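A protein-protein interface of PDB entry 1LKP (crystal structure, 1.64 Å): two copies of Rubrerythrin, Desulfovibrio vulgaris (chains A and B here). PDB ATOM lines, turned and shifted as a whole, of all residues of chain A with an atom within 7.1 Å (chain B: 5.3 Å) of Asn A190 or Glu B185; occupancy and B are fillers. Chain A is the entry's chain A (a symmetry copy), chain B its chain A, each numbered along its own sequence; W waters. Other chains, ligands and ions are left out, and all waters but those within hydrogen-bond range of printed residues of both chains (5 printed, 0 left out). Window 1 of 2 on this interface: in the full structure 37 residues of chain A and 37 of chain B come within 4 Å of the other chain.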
ATOM      1  N   GLU A  48      -8.609 -28.297   8.713  1.00  0.00           N
ATOM      2  CA  GLU A  48      -7.308 -27.710   9.009  1.00  0.00           C
ATOM      3  C   GLU A  48      -6.218 -28.505   8.308  1.00  0.00           C
ATOM      4  O   GLU A  48      -5.282 -27.934   7.754  1.00  0.00           O
ATOM      5  CB  GLU A  48      -7.023 -27.703  10.514  1.00  0.00           C
ATOM      6  CG  GLU A  48      -5.734 -26.948  10.857  1.00  0.00           C
ATOM      7  CD  GLU A  48      -5.182 -27.283  12.233  1.00  0.00           C
ATOM      8  OE1 GLU A  48      -4.838 -28.459  12.462  1.00  0.00           O
ATOM      9  OE2 GLU A  48      -5.078 -26.368  13.081  1.00  0.00           O
ATOM     10  N   GLN A  52      -3.378 -27.336   5.561  1.00  0.00           N
ATOM     11  CA  GLN A  52      -1.949 -27.538   5.725  1.00  0.00           C
ATOM     12  C   GLN A  52      -1.373 -28.261   4.512  1.00  0.00           C
ATOM     13  O   GLN A  52      -0.238 -27.989   4.122  1.00  0.00           O
ATOM     14  CB  GLN A  52      -1.665 -28.270   7.041  1.00  0.00           C
ATOM     15  CG  GLN A  52      -2.152 -27.441   8.235  1.00  0.00           C
ATOM     16  CD  GLN A  52      -1.830 -28.034   9.589  1.00  0.00           C
ATOM     17  OE1 GLN A  52      -1.741 -29.249   9.747  1.00  0.00           O
ATOM     18  NE2 GLN A  52      -1.685 -27.166  10.590  1.00  0.00           N
ATOM     19  N   ARG A 134      -3.177 -37.733  14.616  1.00  0.00           N
ATOM     20  CA  ARG A 134      -4.500 -37.188  14.888  1.00  0.00           C
ATOM     21  C   ARG A 134      -5.584 -38.082  14.299  1.00  0.00           C
ATOM     22  O   ARG A 134      -6.550 -38.426  14.980  1.00  0.00           O
ATOM     23  CB  ARG A 134      -4.642 -35.775  14.315  1.00  0.00           C
ATOM     24  CG  ARG A 134      -3.642 -34.789  14.872  1.00  0.00           C
ATOM     25  CD  ARG A 134      -4.128 -33.354  14.734  1.00  0.00           C
ATOM     26  NE  ARG A 134      -4.248 -32.914  13.346  1.00  0.00           N
ATOM     27  CZ  ARG A 134      -4.483 -31.654  12.997  1.00  0.00           C
ATOM     28  NH1 ARG A 134      -4.619 -30.728  13.938  1.00  0.00           N
ATOM     29  NH2 ARG A 134      -4.582 -31.316  11.719  1.00  0.00           N
ATOM     30  N   GLY A 188      -9.110 -28.100  25.767  1.00  0.00           N
ATOM     31  CA  GLY A 188      -7.670 -28.129  25.603  1.00  0.00           C
ATOM     32  C   GLY A 188      -7.010 -26.800  25.915  1.00  0.00           C
ATOM     33  O   GLY A 188      -7.559 -25.737  25.633  1.00  0.00           O
ATOM     34  N   ILE A 189      -5.822 -26.869  26.503  1.00  0.00           N
ATOM     35  CA  ILE A 189      -5.064 -25.676  26.848  1.00  0.00           C
ATOM     36  C   ILE A 189      -3.629 -25.863  26.369  1.00  0.00           C
ATOM     37  O   ILE A 189      -2.810 -26.458  27.070  1.00  0.00           O
ATOM     38  CB  ILE A 189      -5.060 -25.444  28.375  1.00  0.00           C
ATOM     39  CG1 ILE A 189      -6.483 -25.154  28.857  1.00  0.00           C
ATOM     40  CG2 ILE A 189      -4.126 -24.293  28.728  1.00  0.00           C
ATOM     41  CD1 ILE A 189      -6.625 -25.094  30.368  1.00  0.00           C
ATOM     42  N   ASN A 190      -3.325 -25.375  25.169  1.00  0.00           N
ATOM     43  CA  ASN A 190      -1.973 -25.506  24.644  1.00  0.00           C
ATOM     44  C   ASN A 190      -1.257 -24.162  24.601  1.00  0.00           C
ATOM     45  O   ASN A 190      -0.923 -23.647  23.536  1.00  0.00           O
ATOM     46  CB  ASN A 190      -1.970 -26.172  23.253  1.00  0.00           C
ATOM     47  CG  ASN A 190      -2.729 -25.377  22.197  1.00  0.00           C
ATOM     48  OD1 ASN A 190      -2.365 -25.398  21.017  1.00  0.00           O
ATOM     49  ND2 ASN A 190      -3.789 -24.695  22.603  1.00  0.00           N
ATOM     50  N   TRP A 191      -1.036 -23.600  25.785  1.00  0.00           N
ATOM     51  CA  TRP A 191      -0.352 -22.323  25.941  1.00  0.00           C
ATOM     52  C   TRP A 191       0.098 -22.165  27.391  1.00  0.00           C
ATOM     53  O   TRP A 191      -0.147 -23.101  28.182  1.00  0.00           O
ATOM     54  CB  TRP A 191      -1.284 -21.173  25.541  1.00  0.00           C
ATOM     55  CG  TRP A 191      -2.556 -21.114  26.335  1.00  0.00           C
ATOM     56  CD1 TRP A 191      -2.711 -20.644  27.608  1.00  0.00           C
ATOM     57  CD2 TRP A 191      -3.848 -21.561  25.912  1.00  0.00           C
ATOM     58  NE1 TRP A 191      -4.022 -20.771  28.005  1.00  0.00           N
ATOM     59  CE2 TRP A 191      -4.742 -21.330  26.982  1.00  0.00           C
ATOM     60  CE3 TRP A 191      -4.339 -22.134  24.731  1.00  0.00           C
ATOM     61  CZ2 TRP A 191      -6.101 -21.657  26.909  1.00  0.00           C
ATOM     62  CZ3 TRP A 191      -5.692 -22.459  24.656  1.00  0.00           C
ATOM     63  CH2 TRP A 191      -6.556 -22.218  25.739  1.00  0.00           C
ATOM     64  OXT TRP A 191       0.690 -21.117  27.722  1.00  0.00           O
ATOM     65  N   GLN B  41      -1.387 -17.862  16.608  1.00  0.00           N
ATOM     66  CA  GLN B  41      -2.291 -18.621  17.470  1.00  0.00           C
ATOM     67  C   GLN B  41      -3.255 -17.670  18.165  1.00  0.00           C
ATOM     68  O   GLN B  41      -4.458 -17.923  18.224  1.00  0.00           O
ATOM     69  CB  GLN B  41      -1.537 -19.420  18.536  1.00  0.00           C
ATOM     70  CG  GLN B  41      -2.482 -20.336  19.317  1.00  0.00           C
ATOM     71  CD  GLN B  41      -1.842 -21.029  20.500  1.00  0.00           C
ATOM     72  OE1 GLN B  41      -2.395 -21.995  21.040  1.00  0.00           O
ATOM     73  NE2 GLN B  41      -0.692 -20.539  20.923  1.00  0.00           N
ATOM     74  N   LYS B 155       7.357 -29.552  22.504  1.00  0.00           N
ATOM     75  CA  LYS B 155       6.993 -29.678  21.096  1.00  0.00           C
ATOM     76  C   LYS B 155       6.205 -28.463  20.621  1.00  0.00           C
ATOM     77  O   LYS B 155       5.260 -28.029  21.279  1.00  0.00           O
ATOM     78  CB  LYS B 155       6.170 -30.951  20.866  1.00  0.00           C
ATOM     79  CG  LYS B 155       6.969 -32.238  21.028  1.00  0.00           C
ATOM     80  CD  LYS B 155       6.138 -33.446  20.638  1.00  0.00           C
ATOM     81  CE  LYS B 155       6.967 -34.717  20.661  1.00  0.00           C
ATOM     82  NZ  LYS B 155       6.192 -35.889  20.172  1.00  0.00           N
ATOM     83  N   TRP B 156       6.616 -27.922  19.478  1.00  0.00           N
ATOM     84  CA  TRP B 156       5.976 -26.762  18.870  1.00  0.00           C
ATOM     85  C   TRP B 156       5.382 -27.160  17.524  1.00  0.00           C
ATOM     86  O   TRP B 156       6.020 -27.869  16.748  1.00  0.00           O
ATOM     87  CB  TRP B 156       7.003 -25.650  18.652  1.00  0.00           C
ATOM     88  CG  TRP B 156       7.670 -25.190  19.907  1.00  0.00           C
ATOM     89  CD1 TRP B 156       8.771 -25.737  20.507  1.00  0.00           C
ATOM     90  CD2 TRP B 156       7.266 -24.093  20.732  1.00  0.00           C
ATOM     91  NE1 TRP B 156       9.077 -25.042  21.658  1.00  0.00           N
ATOM     92  CE2 TRP B 156       8.168 -24.029  21.817  1.00  0.00           C
ATOM     93  CE3 TRP B 156       6.225 -23.158  20.659  1.00  0.00           C
ATOM     94  CZ2 TRP B 156       8.061 -23.063  22.825  1.00  0.00           C
ATOM     95  CZ3 TRP B 156       6.118 -22.196  21.662  1.00  0.00           C
ATOM     96  CH2 TRP B 156       7.033 -22.158  22.730  1.00  0.00           C
ATOM     97  N   ARG B 157       4.166 -26.707  17.241  1.00  0.00           N
ATOM     98  CA  ARG B 157       3.533 -27.043  15.969  1.00  0.00           C
ATOM     99  C   ARG B 157       3.332 -25.799  15.115  1.00  0.00           C
ATOM    100  O   ARG B 157       2.932 -24.747  15.617  1.00  0.00           O
ATOM    101  CB  ARG B 157       2.172 -27.716  16.199  1.00  0.00           C
ATOM    102  CG  ARG B 157       1.548 -28.278  14.917  1.00  0.00           C
ATOM    103  CD  ARG B 157       0.124 -28.791  15.136  1.00  0.00           C
ATOM    104  NE  ARG B 157      -0.836 -27.707  15.347  1.00  0.00           N
ATOM    105  CZ  ARG B 157      -1.926 -27.517  14.609  1.00  0.00           C
ATOM    106  NH1 ARG B 157      -2.201 -28.339  13.604  1.00  0.00           N
ATOM    107  NH2 ARG B 157      -2.746 -26.508  14.877  1.00  0.00           N
ATOM    108  N   CYS B 158       3.633 -25.917  13.827  1.00  0.00           N
ATOM    109  CA  CYS B 158       3.444 -24.804  12.902  1.00  0.00           C
ATOM    110  C   CYS B 158       1.971 -24.834  12.500  1.00  0.00           C
ATOM    111  O   CYS B 158       1.510 -25.807  11.907  1.00  0.00           O
ATOM    112  CB  CYS B 158       4.315 -24.985  11.658  1.00  0.00           C
ATOM    113  SG  CYS B 158       3.996 -23.764  10.363  1.00  0.00           S
ATOM    114  N   ARG B 159       1.229 -23.783  12.825  1.00  0.00           N
ATOM    115  CA  ARG B 159      -0.187 -23.750  12.470  1.00  0.00           C
ATOM    116  C   ARG B 159      -0.405 -23.708  10.953  1.00  0.00           C
ATOM    117  O   ARG B 159      -1.441 -24.155  10.458  1.00  0.00           O
ATOM    118  CB  ARG B 159      -0.877 -22.548  13.134  1.00  0.00           C
ATOM    119  CG  ARG B 159      -1.050 -22.691  14.648  1.00  0.00           C
ATOM    120  CD  ARG B 159      -1.811 -21.508  15.248  1.00  0.00           C
ATOM    121  NE  ARG B 159      -3.179 -21.403  14.740  1.00  0.00           N
ATOM    122  CZ  ARG B 159      -4.172 -22.235  15.055  1.00  0.00           C
ATOM    123  NH1 ARG B 159      -3.969 -23.246  15.892  1.00  0.00           N
ATOM    124  NH2 ARG B 159      -5.373 -22.064  14.517  1.00  0.00           N
ATOM    125  N   HIS B 183       3.818 -18.330  13.321  1.00  0.00           N
ATOM    126  CA  HIS B 183       2.839 -19.391  13.115  1.00  0.00           C
ATOM    127  C   HIS B 183       2.898 -20.547  14.111  1.00  0.00           C
ATOM    128  O   HIS B 183       2.017 -21.406  14.113  1.00  0.00           O
ATOM    129  CB  HIS B 183       2.977 -19.934  11.692  1.00  0.00           C
ATOM    130  CG  HIS B 183       2.585 -18.949  10.638  1.00  0.00           C
ATOM    131  ND1 HIS B 183       1.319 -18.906  10.094  1.00  0.00           N
ATOM    132  CD2 HIS B 183       3.273 -17.929  10.073  1.00  0.00           C
ATOM    133  CE1 HIS B 183       1.245 -17.899   9.240  1.00  0.00           C
ATOM    134  NE2 HIS B 183       2.417 -17.290   9.210  1.00  0.00           N
ATOM    135  N   PHE B 184       3.913 -20.565  14.969  1.00  0.00           N
ATOM    136  CA  PHE B 184       4.047 -21.659  15.924  1.00  0.00           C
ATOM    137  C   PHE B 184       3.276 -21.540  17.231  1.00  0.00           C
ATOM    138  O   PHE B 184       3.029 -20.447  17.743  1.00  0.00           O
ATOM    139  CB  PHE B 184       5.527 -21.913  16.233  1.00  0.00           C
ATOM    140  CG  PHE B 184       6.268 -22.603  15.120  1.00  0.00           C
ATOM    141  CD1 PHE B 184       6.778 -21.877  14.047  1.00  0.00           C
ATOM    142  CD2 PHE B 184       6.421 -23.991  15.126  1.00  0.00           C
ATOM    143  CE1 PHE B 184       7.429 -22.521  12.991  1.00  0.00           C
ATOM    144  CE2 PHE B 184       7.071 -24.647  14.073  1.00  0.00           C
ATOM    145  CZ  PHE B 184       7.574 -23.907  13.006  1.00  0.00           C
ATOM    146  N   GLU B 185       2.903 -22.700  17.762  1.00  0.00           N
ATOM    147  CA  GLU B 185       2.165 -22.802  19.015  1.00  0.00           C
ATOM    148  C   GLU B 185       2.645 -24.059  19.718  1.00  0.00           C
ATOM    149  O   GLU B 185       3.300 -24.907  19.111  1.00  0.00           O
ATOM    150  CB  GLU B 185       0.665 -22.944  18.740  1.00  0.00           C
ATOM    151  CG  GLU B 185       0.326 -24.228  17.972  1.00  0.00           C
ATOM    152  CD  GLU B 185      -1.160 -24.420  17.742  1.00  0.00           C
ATOM    153  OE1 GLU B 185      -1.925 -23.450  17.918  1.00  0.00           O
ATOM    154  OE2 GLU B 185      -1.559 -25.547  17.371  1.00  0.00           O
ATOM    155  N   LEU B 186       2.339 -24.180  21.002  1.00  0.00           N
ATOM    156  CA  LEU B 186       2.710 -25.388  21.721  1.00  0.00           C
ATOM    157  C   LEU B 186       1.826 -26.482  21.137  1.00  0.00           C
ATOM    158  O   LEU B 186       0.632 -26.268  20.924  1.00  0.00           O
ATOM    159  CB  LEU B 186       2.423 -25.240  23.217  1.00  0.00           C
ATOM    160  CG  LEU B 186       3.364 -24.348  24.024  1.00  0.00           C
ATOM    161  CD1 LEU B 186       2.884 -24.284  25.471  1.00  0.00           C
ATOM    162  CD2 LEU B 186       4.781 -24.906  23.955  1.00  0.00           C
ATOM    163  N   LEU B 187       2.410 -27.642  20.863  1.00  0.00           N
ATOM    164  CA  LEU B 187       1.647 -28.752  20.306  1.00  0.00           C
ATOM    165  C   LEU B 187       0.602 -29.182  21.323  1.00  0.00           C
ATOM    166  O   LEU B 187       0.935 -29.516  22.461  1.00  0.00           O
ATOM    167  CB  LEU B 187       2.583 -29.922  19.984  1.00  0.00           C
ATOM    168  CG  LEU B 187       2.020 -31.160  19.271  1.00  0.00           C
ATOM    169  CD1 LEU B 187       1.074 -31.914  20.184  1.00  0.00           C
ATOM    170  CD2 LEU B 187       1.321 -30.738  17.995  1.00  0.00           C
ATOM    171  N   GLY B 188      -0.660 -29.165  20.913  1.00  0.00           N
ATOM    172  CA  GLY B 188      -1.731 -29.551  21.810  1.00  0.00           C
ATOM    173  C   GLY B 188      -2.462 -30.801  21.360  1.00  0.00           C
ATOM    174  O   GLY B 188      -2.654 -31.028  20.167  1.00  0.00           O
HETATM  175  O   HOH W   1       1.055 -21.983  22.531  1.00  0.00           O
HETATM  176  O   HOH W   2      -6.917 -24.409  13.169  1.00  0.00           O
HETATM  177  O   HOH W   3      -4.292 -25.398  18.348  1.00  0.00           O
HETATM  178  O   HOH W   4      -1.254 -30.602  12.250  1.00  0.00           O
HETATM  179  O   HOH W   5      -3.995 -23.788  11.565  1.00  0.00           O
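O of Arg B159 sits at hydrogen-bond distance from NE2 of Gln A52 (3.0 Å). The side-chain carboxylate (OE1) of Glu A48 is in salt-bridge range of the guanidinium group (NH1) of Arg B157. The guanidinium group of Arg A134 sits close to the guanidinium group of Arg B157 (3.4 Å). The side-chain amide nitrogen of Gln A52 sits close to the guanidinium group of Arg B157. OD1 of Asn A190 lies close to O of Leu B186, 3.1 Å away. O of Asn A190 lies close to OE1 of Gln B41 (3.3 Å).
1 position is printed for both chains.
Water W2 bridges OE2 of Glu A48 (2.7 Å) and NH2 of Arg B159 (3.1 Å). Water W1 lies within hydrogen-bond range of O of Asn A190 (2.8 Å), NE2 of Gln B41 (2.8 Å) and N of Leu B186 (3.0 Å). Water W4 lies within hydrogen-bond range of NH1 of Arg B157 (2.8 Å), OE1 of Gln A52 (2.9 Å) and NH2 of Arg A134 (3.4 Å). Water W5 bridges O of Arg B159 (2.8 Å) and OE2 of Glu A48 (3.2 Å). Water W3 lies within hydrogen-bond range of the side-chain carboxylate (OE2) of Glu B185, the guanidinium group (NH1) of Arg B159 and the side-chain amide oxygen (OD1) of Asn A190.
Of the 12 printed residues of chain B, 7 touch a printed residue of chain A. Hydrophobic or aromatic side chains of chain B within 4 Å of the printed part of chain A: Leu B186. Of the 7 printed residues of chain A, 5 touch a printed residue of chain B. Among the printed residues, 10 pairs touch across the chains. Among the printed residues, Asp or Glu carboxylates within 4 Å of a Lys or Arg side-chain nitrogen of the other chain: Glu A48 with Arg B157 (2.9 Å).
Asn A190 touches just these residues of chain B: Gln B41 (3.3 Å), Glu B185 (3.6 Å), Leu B186 (3.1 Å) and Gly B188 (3.7 Å). Of the printed residues of chain B, Trp A191 touches Leu B186 (3.8 Å). Of the printed residues of chain A, Gln B41 touches Asn A190. Of the printed residues of chain A, Arg B159 touches Gln A52 (3.0 Å). His B183 touches none of the printed residues of chain A. Glu B185 touches just one residue of chain A: Asn A190 (3.6 Å). The nearest printed residue of chain A that does not touch Gln B41 is Trp A191 (4.2 Å).
The backbone NH of Arg B159 sits at hydrogen-bond distance from the backbone carbonyl oxygen of His B183 (2.8 Å). The guanidinium group (NH1) of Arg A134 lies within salt-bridge range of the side-chain carboxylate (OE1) of Glu A48 (2.7 Å). The guanidinium group of Arg B159 lies within salt-bridge range of the side-chain carboxylate of Glu B185. The side-chain amide oxygen (OE1) of Gln B41 lies close to the side-chain carboxylate (OE1) of Glu B185 (3.5 Å). The guanidinium group (NH2) of Arg B157 is in salt-bridge range of the side-chain carboxylate (OE2) of Glu B185 (2.9 Å).
NE2 of Gln A52 touches O of Cys B158, 3.7 Å away. Glu B185 touches Asn A190 (CD to OD1, 3.6 Å). Asn A190 touches Gly B188. Trp A191 touches Leu B186.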
